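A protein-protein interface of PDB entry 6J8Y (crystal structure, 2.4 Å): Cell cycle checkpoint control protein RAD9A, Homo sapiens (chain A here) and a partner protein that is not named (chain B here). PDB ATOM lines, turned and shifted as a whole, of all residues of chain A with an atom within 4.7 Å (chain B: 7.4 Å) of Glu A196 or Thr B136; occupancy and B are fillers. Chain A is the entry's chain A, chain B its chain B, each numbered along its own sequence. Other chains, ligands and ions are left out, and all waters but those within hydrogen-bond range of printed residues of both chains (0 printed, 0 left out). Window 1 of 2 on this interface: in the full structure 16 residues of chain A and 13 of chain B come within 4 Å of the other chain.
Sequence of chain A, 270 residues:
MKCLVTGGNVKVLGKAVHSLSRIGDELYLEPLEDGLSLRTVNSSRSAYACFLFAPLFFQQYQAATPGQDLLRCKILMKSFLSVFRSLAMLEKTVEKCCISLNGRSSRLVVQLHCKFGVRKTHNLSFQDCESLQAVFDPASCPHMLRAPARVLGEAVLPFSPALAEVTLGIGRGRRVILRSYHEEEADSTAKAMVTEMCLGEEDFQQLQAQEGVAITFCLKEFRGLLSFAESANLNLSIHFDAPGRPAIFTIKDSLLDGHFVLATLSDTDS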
ATOM      1  N   ILE A 177     -26.901 -19.661  35.429  1.00  0.00           N
ATOM      2  CA  ILE A 177     -25.792 -19.202  34.597  1.00  0.00           C
ATOM      3  C   ILE A 177     -24.832 -20.326  34.216  1.00  0.00           C
ATOM      4  O   ILE A 177     -24.369 -21.078  35.073  1.00  0.00           O
ATOM      5  CB  ILE A 177     -24.982 -18.097  35.306  1.00  0.00           C
ATOM      6  CG1 ILE A 177     -25.915 -17.052  35.921  1.00  0.00           C
ATOM      7  CG2 ILE A 177     -23.997 -17.455  34.341  1.00  0.00           C
ATOM      8  CD1 ILE A 177     -26.697 -16.262  34.903  1.00  0.00           C
ATOM      9  N   LEU A 178     -24.536 -20.428  32.925  1.00  0.00           N
ATOM     10  CA  LEU A 178     -23.496 -21.330  32.443  1.00  0.00           C
ATOM     11  C   LEU A 178     -22.335 -20.513  31.886  1.00  0.00           C
ATOM     12  O   LEU A 178     -22.469 -19.851  30.858  1.00  0.00           O
ATOM     13  CB  LEU A 178     -24.043 -22.278  31.372  1.00  0.00           C
ATOM     14  CG  LEU A 178     -24.057 -23.770  31.711  1.00  0.00           C
ATOM     15  CD1 LEU A 178     -24.972 -24.047  32.890  1.00  0.00           C
ATOM     16  CD2 LEU A 178     -24.473 -24.596  30.503  1.00  0.00           C
ATOM     17  N   ARG A 179     -21.197 -20.557  32.570  1.00  0.00           N
ATOM     18  CA  ARG A 179     -20.035 -19.774  32.161  1.00  0.00           C
ATOM     19  C   ARG A 179     -18.797 -20.643  31.963  1.00  0.00           C
ATOM     20  O   ARG A 179     -18.497 -21.511  32.783  1.00  0.00           O
ATOM     21  CB  ARG A 179     -19.740 -18.683  33.193  1.00  0.00           C
ATOM     22  CG  ARG A 179     -18.476 -17.890  32.910  1.00  0.00           C
ATOM     23  CD  ARG A 179     -18.168 -16.896  34.019  1.00  0.00           C
ATOM     24  NE  ARG A 179     -19.250 -15.938  34.219  1.00  0.00           N
ATOM     25  CZ  ARG A 179     -20.106 -15.976  35.236  1.00  0.00           C
ATOM     26  NH1 ARG A 179     -20.007 -16.930  36.153  1.00  0.00           N
ATOM     27  NH2 ARG A 179     -21.060 -15.061  35.336  1.00  0.00           N
ATOM     28  N   VAL A 194     -14.444 -15.436  27.175  1.00  0.00           N
ATOM     29  CA  VAL A 194     -15.372 -16.092  28.085  1.00  0.00           C
ATOM     30  C   VAL A 194     -16.776 -16.099  27.487  1.00  0.00           C
ATOM     31  O   VAL A 194     -17.252 -15.097  26.949  1.00  0.00           O
ATOM     32  CB  VAL A 194     -15.382 -15.422  29.482  1.00  0.00           C
ATOM     33  CG1 VAL A 194     -14.002 -15.511  30.117  1.00  0.00           C
ATOM     34  CG2 VAL A 194     -15.822 -13.976  29.395  1.00  0.00           C
ATOM     35  N   THR A 195     -17.422 -17.257  27.555  1.00  0.00           N
ATOM     36  CA  THR A 195     -18.781 -17.409  27.057  1.00  0.00           C
ATOM     37  C   THR A 195     -19.723 -17.649  28.227  1.00  0.00           C
ATOM     38  O   THR A 195     -19.428 -18.449  29.115  1.00  0.00           O
ATOM     39  CB  THR A 195     -18.890 -18.569  26.047  1.00  0.00           C
ATOM     40  OG1 THR A 195     -18.068 -18.292  24.907  1.00  0.00           O
ATOM     41  CG2 THR A 195     -20.333 -18.761  25.593  1.00  0.00           C
ATOM     42  N   GLU A 196     -20.848 -16.942  28.233  1.00  0.00           N
ATOM     43  CA  GLU A 196     -21.831 -17.107  29.292  1.00  0.00           C
ATOM     44  C   GLU A 196     -23.242 -17.255  28.740  1.00  0.00           C
ATOM     45  O   GLU A 196     -23.745 -16.377  28.040  1.00  0.00           O
ATOM     46  CB  GLU A 196     -21.777 -15.926  30.263  1.00  0.00           C
ATOM     47  CG  GLU A 196     -22.973 -15.851  31.195  1.00  0.00           C
ATOM     48  CD  GLU A 196     -22.795 -14.824  32.294  1.00  0.00           C
ATOM     49  OE1 GLU A 196     -21.656 -14.665  32.780  1.00  0.00           O
ATOM     50  OE2 GLU A 196     -23.794 -14.176  32.671  1.00  0.00           O
ATOM     51  N   MET A 197     -23.872 -18.382  29.056  1.00  0.00           N
ATOM     52  CA  MET A 197     -25.271 -18.601  28.721  1.00  0.00           C
ATOM     53  C   MET A 197     -26.140 -18.335  29.941  1.00  0.00           C
ATOM     54  O   MET A 197     -25.910 -18.897  31.011  1.00  0.00           O
ATOM     55  CB  MET A 197     -25.496 -20.027  28.214  1.00  0.00           C
ATOM     56  CG  MET A 197     -26.959 -20.439  28.170  1.00  0.00           C
ATOM     57  SD  MET A 197     -27.889 -19.654  26.837  1.00  0.00           S
ATOM     58  CE  MET A 197     -27.500 -20.740  25.467  1.00  0.00           C
ATOM     59  N   CYS A 198     -27.135 -17.470  29.780  1.00  0.00           N
ATOM     60  CA  CYS A 198     -28.047 -17.156  30.870  1.00  0.00           C
ATOM     61  C   CYS A 198     -29.427 -17.750  30.609  1.00  0.00           C
ATOM     62  O   CYS A 198     -30.067 -17.445  29.603  1.00  0.00           O
ATOM     63  CB  CYS A 198     -28.150 -15.644  31.070  1.00  0.00           C
ATOM     64  SG  CYS A 198     -29.113 -15.153  32.519  1.00  0.00           S
ATOM     65  N   ALA B  97     -18.209 -16.628  18.380  1.00  0.00           N
ATOM     66  CA  ALA B  97     -19.190 -15.765  19.024  1.00  0.00           C
ATOM     67  C   ALA B  97     -20.384 -15.508  18.112  1.00  0.00           C
ATOM     68  O   ALA B  97     -21.531 -15.520  18.558  1.00  0.00           O
ATOM     69  CB  ALA B  97     -18.547 -14.449  19.434  1.00  0.00           C
ATOM     70  N   THR B 100     -23.387 -18.303  17.279  1.00  0.00           N
ATOM     71  CA  THR B 100     -24.639 -18.261  18.024  1.00  0.00           C
ATOM     72  C   THR B 100     -25.535 -17.126  17.541  1.00  0.00           C
ATOM     73  O   THR B 100     -26.758 -17.195  17.659  1.00  0.00           O
ATOM     74  CB  THR B 100     -24.387 -18.094  19.536  1.00  0.00           C
ATOM     75  OG1 THR B 100     -23.278 -17.210  19.744  1.00  0.00           O
ATOM     76  CG2 THR B 100     -24.069 -19.434  20.168  1.00  0.00           C
ATOM     77  N   LYS B 114     -14.219  -4.895  31.796  1.00  0.00           N
ATOM     78  CA  LYS B 114     -14.510  -5.450  33.114  1.00  0.00           C
ATOM     79  C   LYS B 114     -13.243  -5.997  33.761  1.00  0.00           C
ATOM     80  O   LYS B 114     -12.696  -5.399  34.688  1.00  0.00           O
ATOM     81  CB  LYS B 114     -15.568  -6.545  32.996  1.00  0.00           C
ATOM     82  CG  LYS B 114     -16.577  -6.286  31.888  1.00  0.00           C
ATOM     83  CD  LYS B 114     -17.322  -7.551  31.494  1.00  0.00           C
ATOM     84  CE  LYS B 114     -18.067  -7.356  30.182  1.00  0.00           C
ATOM     85  NZ  LYS B 114     -19.146  -8.363  29.990  1.00  0.00           N
ATOM     86  N   THR B 120     -17.628  -7.110  23.616  1.00  0.00           N
ATOM     87  CA  THR B 120     -18.673  -8.005  24.093  1.00  0.00           C
ATOM     88  C   THR B 120     -19.750  -8.225  23.041  1.00  0.00           C
ATOM     89  O   THR B 120     -20.344  -7.276  22.529  1.00  0.00           O
ATOM     90  CB  THR B 120     -19.324  -7.471  25.378  1.00  0.00           C
ATOM     91  OG1 THR B 120     -18.346  -7.424  26.423  1.00  0.00           O
ATOM     92  CG2 THR B 120     -20.469  -8.372  25.805  1.00  0.00           C
ATOM     93  N   VAL B 121     -19.993  -9.491  22.726  1.00  0.00           N
ATOM     94  CA  VAL B 121     -21.020  -9.868  21.767  1.00  0.00           C
ATOM     95  C   VAL B 121     -22.209 -10.493  22.493  1.00  0.00           C
ATOM     96  O   VAL B 121     -22.137 -11.631  22.959  1.00  0.00           O
ATOM     97  CB  VAL B 121     -20.465 -10.852  20.716  1.00  0.00           C
ATOM     98  CG1 VAL B 121     -21.579 -11.390  19.842  1.00  0.00           C
ATOM     99  CG2 VAL B 121     -19.397 -10.172  19.869  1.00  0.00           C
ATOM    100  N   SER B 122     -23.296  -9.737  22.603  1.00  0.00           N
ATOM    101  CA  SER B 122     -24.510 -10.237  23.239  1.00  0.00           C
ATOM    102  C   SER B 122     -25.485 -10.759  22.195  1.00  0.00           C
ATOM    103  O   SER B 122     -25.760 -10.091  21.198  1.00  0.00           O
ATOM    104  CB  SER B 122     -25.172  -9.147  24.083  1.00  0.00           C
ATOM    105  OG  SER B 122     -24.470  -8.950  25.297  1.00  0.00           O
ATOM    106  N   VAL B 123     -26.004 -11.958  22.432  1.00  0.00           N
ATOM    107  CA  VAL B 123     -26.894 -12.613  21.482  1.00  0.00           C
ATOM    108  C   VAL B 123     -28.215 -13.009  22.136  1.00  0.00           C
ATOM    109  O   VAL B 123     -28.236 -13.786  23.090  1.00  0.00           O
ATOM    110  CB  VAL B 123     -26.231 -13.862  20.877  1.00  0.00           C
ATOM    111  CG1 VAL B 123     -27.207 -14.602  19.984  1.00  0.00           C
ATOM    112  CG2 VAL B 123     -24.978 -13.478  20.108  1.00  0.00           C
ATOM    113  N   ARG B 133     -33.193 -16.245  26.235  1.00  0.00           N
ATOM    114  CA  ARG B 133     -31.841 -16.701  26.529  1.00  0.00           C
ATOM    115  C   ARG B 133     -30.782 -15.774  25.944  1.00  0.00           C
ATOM    116  O   ARG B 133     -30.767 -15.506  24.742  1.00  0.00           O
ATOM    117  CB  ARG B 133     -31.639 -18.120  26.002  1.00  0.00           C
ATOM    118  CG  ARG B 133     -32.511 -19.144  26.695  1.00  0.00           C
ATOM    119  CD  ARG B 133     -32.505 -20.467  25.961  1.00  0.00           C
ATOM    120  NE  ARG B 133     -33.370 -21.442  26.616  1.00  0.00           N
ATOM    121  CZ  ARG B 133     -33.676 -22.628  26.105  1.00  0.00           C
ATOM    122  NH1 ARG B 133     -33.187 -22.986  24.927  1.00  0.00           N
ATOM    123  NH2 ARG B 133     -34.473 -23.454  26.770  1.00  0.00           N
ATOM    124  N   ILE B 134     -29.894 -15.294  26.808  1.00  0.00           N
ATOM    125  CA  ILE B 134     -28.827 -14.396  26.394  1.00  0.00           C
ATOM    126  C   ILE B 134     -27.481 -15.109  26.397  1.00  0.00           C
ATOM    127  O   ILE B 134     -27.109 -15.743  27.384  1.00  0.00           O
ATOM    128  CB  ILE B 134     -28.735 -13.161  27.313  1.00  0.00           C
ATOM    129  CG1 ILE B 134     -30.128 -12.607  27.621  1.00  0.00           C
ATOM    130  CG2 ILE B 134     -27.841 -12.097  26.690  1.00  0.00           C
ATOM    131  CD1 ILE B 134     -30.886 -12.140  26.397  1.00  0.00           C
ATOM    132  N   VAL B 135     -26.757 -15.007  25.288  1.00  0.00           N
ATOM    133  CA  VAL B 135     -25.400 -15.531  25.218  1.00  0.00           C
ATOM    134  C   VAL B 135     -24.408 -14.382  25.096  1.00  0.00           C
ATOM    135  O   VAL B 135     -24.475 -13.588  24.158  1.00  0.00           O
ATOM    136  CB  VAL B 135     -25.214 -16.494  24.036  1.00  0.00           C
ATOM    137  CG1 VAL B 135     -23.827 -17.110  24.077  1.00  0.00           C
ATOM    138  CG2 VAL B 135     -26.270 -17.579  24.071  1.00  0.00           C
ATOM    139  N   THR B 136     -23.488 -14.300  26.050  1.00  0.00           N
ATOM    140  CA  THR B 136     -22.509 -13.222  26.071  1.00  0.00           C
ATOM    141  C   THR B 136     -21.093 -13.738  25.835  1.00  0.00           C
ATOM    142  O   THR B 136     -20.582 -14.555  26.602  1.00  0.00           O
ATOM    143  CB  THR B 136     -22.552 -12.458  27.408  1.00  0.00           C
ATOM    144  OG1 THR B 136     -23.814 -11.791  27.536  1.00  0.00           O
ATOM    145  CG2 THR B 136     -21.436 -11.430  27.474  1.00  0.00           C
ATOM    146  N   HIS B 137     -20.468 -13.261  24.762  1.00  0.00           N
ATOM    147  CA  HIS B 137     -19.071 -13.575  24.487  1.00  0.00           C
ATOM    148  C   HIS B 137     -18.212 -12.332  24.674  1.00  0.00           C
ATOM    149  O   HIS B 137     -18.421 -11.321  24.006  1.00  0.00           O
ATOM    150  CB  HIS B 137     -18.889 -14.112  23.065  1.00  0.00           C
ATOM    151  CG  HIS B 137     -19.841 -15.204  22.692  1.00  0.00           C
ATOM    152  ND1 HIS B 137     -19.592 -16.534  22.956  1.00  0.00           N
ATOM    153  CD2 HIS B 137     -21.031 -15.166  22.048  1.00  0.00           C
ATOM    154  CE1 HIS B 137     -20.594 -17.266  22.505  1.00  0.00           C
ATOM    155  NE2 HIS B 137     -21.481 -16.460  21.946  1.00  0.00           N
ATOM    156  N   ASP B 138     -17.247 -12.404  25.582  1.00  0.00           N
ATOM    157  CA  ASP B 138     -16.332 -11.292  25.792  1.00  0.00           C
ATOM    158  C   ASP B 138     -15.035 -11.518  25.028  1.00  0.00           C
ATOM    159  O   ASP B 138     -14.124 -12.189  25.512  1.00  0.00           O
ATOM    160  CB  ASP B 138     -16.051 -11.098  27.282  1.00  0.00           C
ATOM    161  CG  ASP B 138     -17.304 -10.762  28.068  1.00  0.00           C
ATOM    162  OD1 ASP B 138     -18.142  -9.995  27.549  1.00  0.00           O
ATOM    163  OD2 ASP B 138     -17.456 -11.267  29.201  1.00  0.00           O
ATOM    164  N   ILE B 139     -14.968 -10.958  23.824  1.00  0.00           N
ATOM    165  CA  ILE B 139     -13.797 -11.092  22.966  1.00  0.00           C
ATOM    166  C   ILE B 139     -12.677 -10.158  23.405  1.00  0.00           C
ATOM    167  O   ILE B 139     -12.827  -8.938  23.334  1.00  0.00           O
ATOM    168  CB  ILE B 139     -14.141 -10.787  21.496  1.00  0.00           C
ATOM    169  CG1 ILE B 139     -15.364 -11.590  21.051  1.00  0.00           C
ATOM    170  CG2 ILE B 139     -12.943 -11.063  20.598  1.00  0.00           C
ATOM    171  CD1 ILE B 139     -15.770 -11.327  19.621  1.00  0.00           C
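The side-chain hydroxyl (OG1) of Thr A195 sits at hydrogen-bond distance from a ring nitrogen (ND1) of His B137 (3.0 Å).
The backbone carbonyl oxygen (O) of Glu A196 sits close to the backbone carbonyl oxygen (O) of Ile B134 (3.5 Å).
O of Glu A196 lies within hydrogen-bond range of N of Thr B136 (2.9 Å).
The backbone carbonyl oxygen (O) of Val A194 lies within hydrogen-bond range of the backbone NH (N) of Asp B138.
The backbone carbonyl oxygen of Thr B136 lies close to the backbone carbonyl oxygen of Val A194, 3.4 Å away.
The backbone NH (N) of Cys A198 lies within hydrogen-bond range of the backbone carbonyl oxygen (O) of Ile B134 (3.0 Å).
N of Val B121 is in hydrogen-bond range of O of His B137, 2.7 Å away.
OG1 of Thr B120 is in hydrogen-bond range of OD1 of Asp B138, 2.8 Å away.
The backbone NH (N) of Met A197 is in hydrogen-bond range of the backbone carbonyl oxygen (O) of Leu A178 (2.7 Å).
The side-chain amino group of Lys B114 lies within salt-bridge range of the side-chain carboxylate of Asp B138 (3.1 Å).
NH2 of Arg A179 lies within salt-bridge range of OE1 of Glu A196, 2.7 Å away.
The side-chain hydroxyl (OG1) of Thr B100 lies within hydrogen-bond range of a ring nitrogen (NE2) of His B137.
CA of His B137 touches O of Val A194, at 3.4 Å.
CA of Thr A195 touches O of Thr B136 (3.4 Å).
Glu A196 touches Val B135.
Met A197 touches Ile B134 (CA to O, 3.7 Å).
CE of Met A197 touches CG2 of Val B135, 3.7 Å away.
Cys A198 touches Arg B133.
Glu A196 touches just these residues of chain B: Ile B134, Val B135 and Thr B136.
Of the printed residues of chain B, Met A197 touches Ile B134 and Val B135.
Ala B97 touches none of the printed residues of chain A.
Of the printed residues of chain A, Ile B134 touches Glu A196, Met A197 and Cys A198.
Of the printed residues of chain A, Val B135 touches Glu A196 (3.4 Å) and Met A197 (3.7 Å).
Thr B136 touches three residues of chain A.
Printed residues of chain A within 4 Å of Asp B138: Val A194.
Ile B139 touches none of the printed residues of chain A.
The nearest residue of chain B that does not touch Glu A196 is His B137 (5.1 Å).
The nearest printed residue of chain A that does not touch Thr B136 is Met A197 (5.1 Å).
The nearest printed residue of chain A that does not touch Val B135 is Thr A195 (4.2 Å).
Hydrophobic or aromatic side chains of chain A within 4 Å of the printed part of chain B: Val A194 and Met A197.
Along chain A the printed residues that touch a printed residue of chain B span positions 194 to 198.
Hydrophobic or aromatic side chains of chain B that line the printed part of chain A: Val B135 and His B137.
Among the printed residues, no Asp or Glu carboxylate lies within 4 Å of a Lys or Arg side-chain nitrogen of the other chain.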
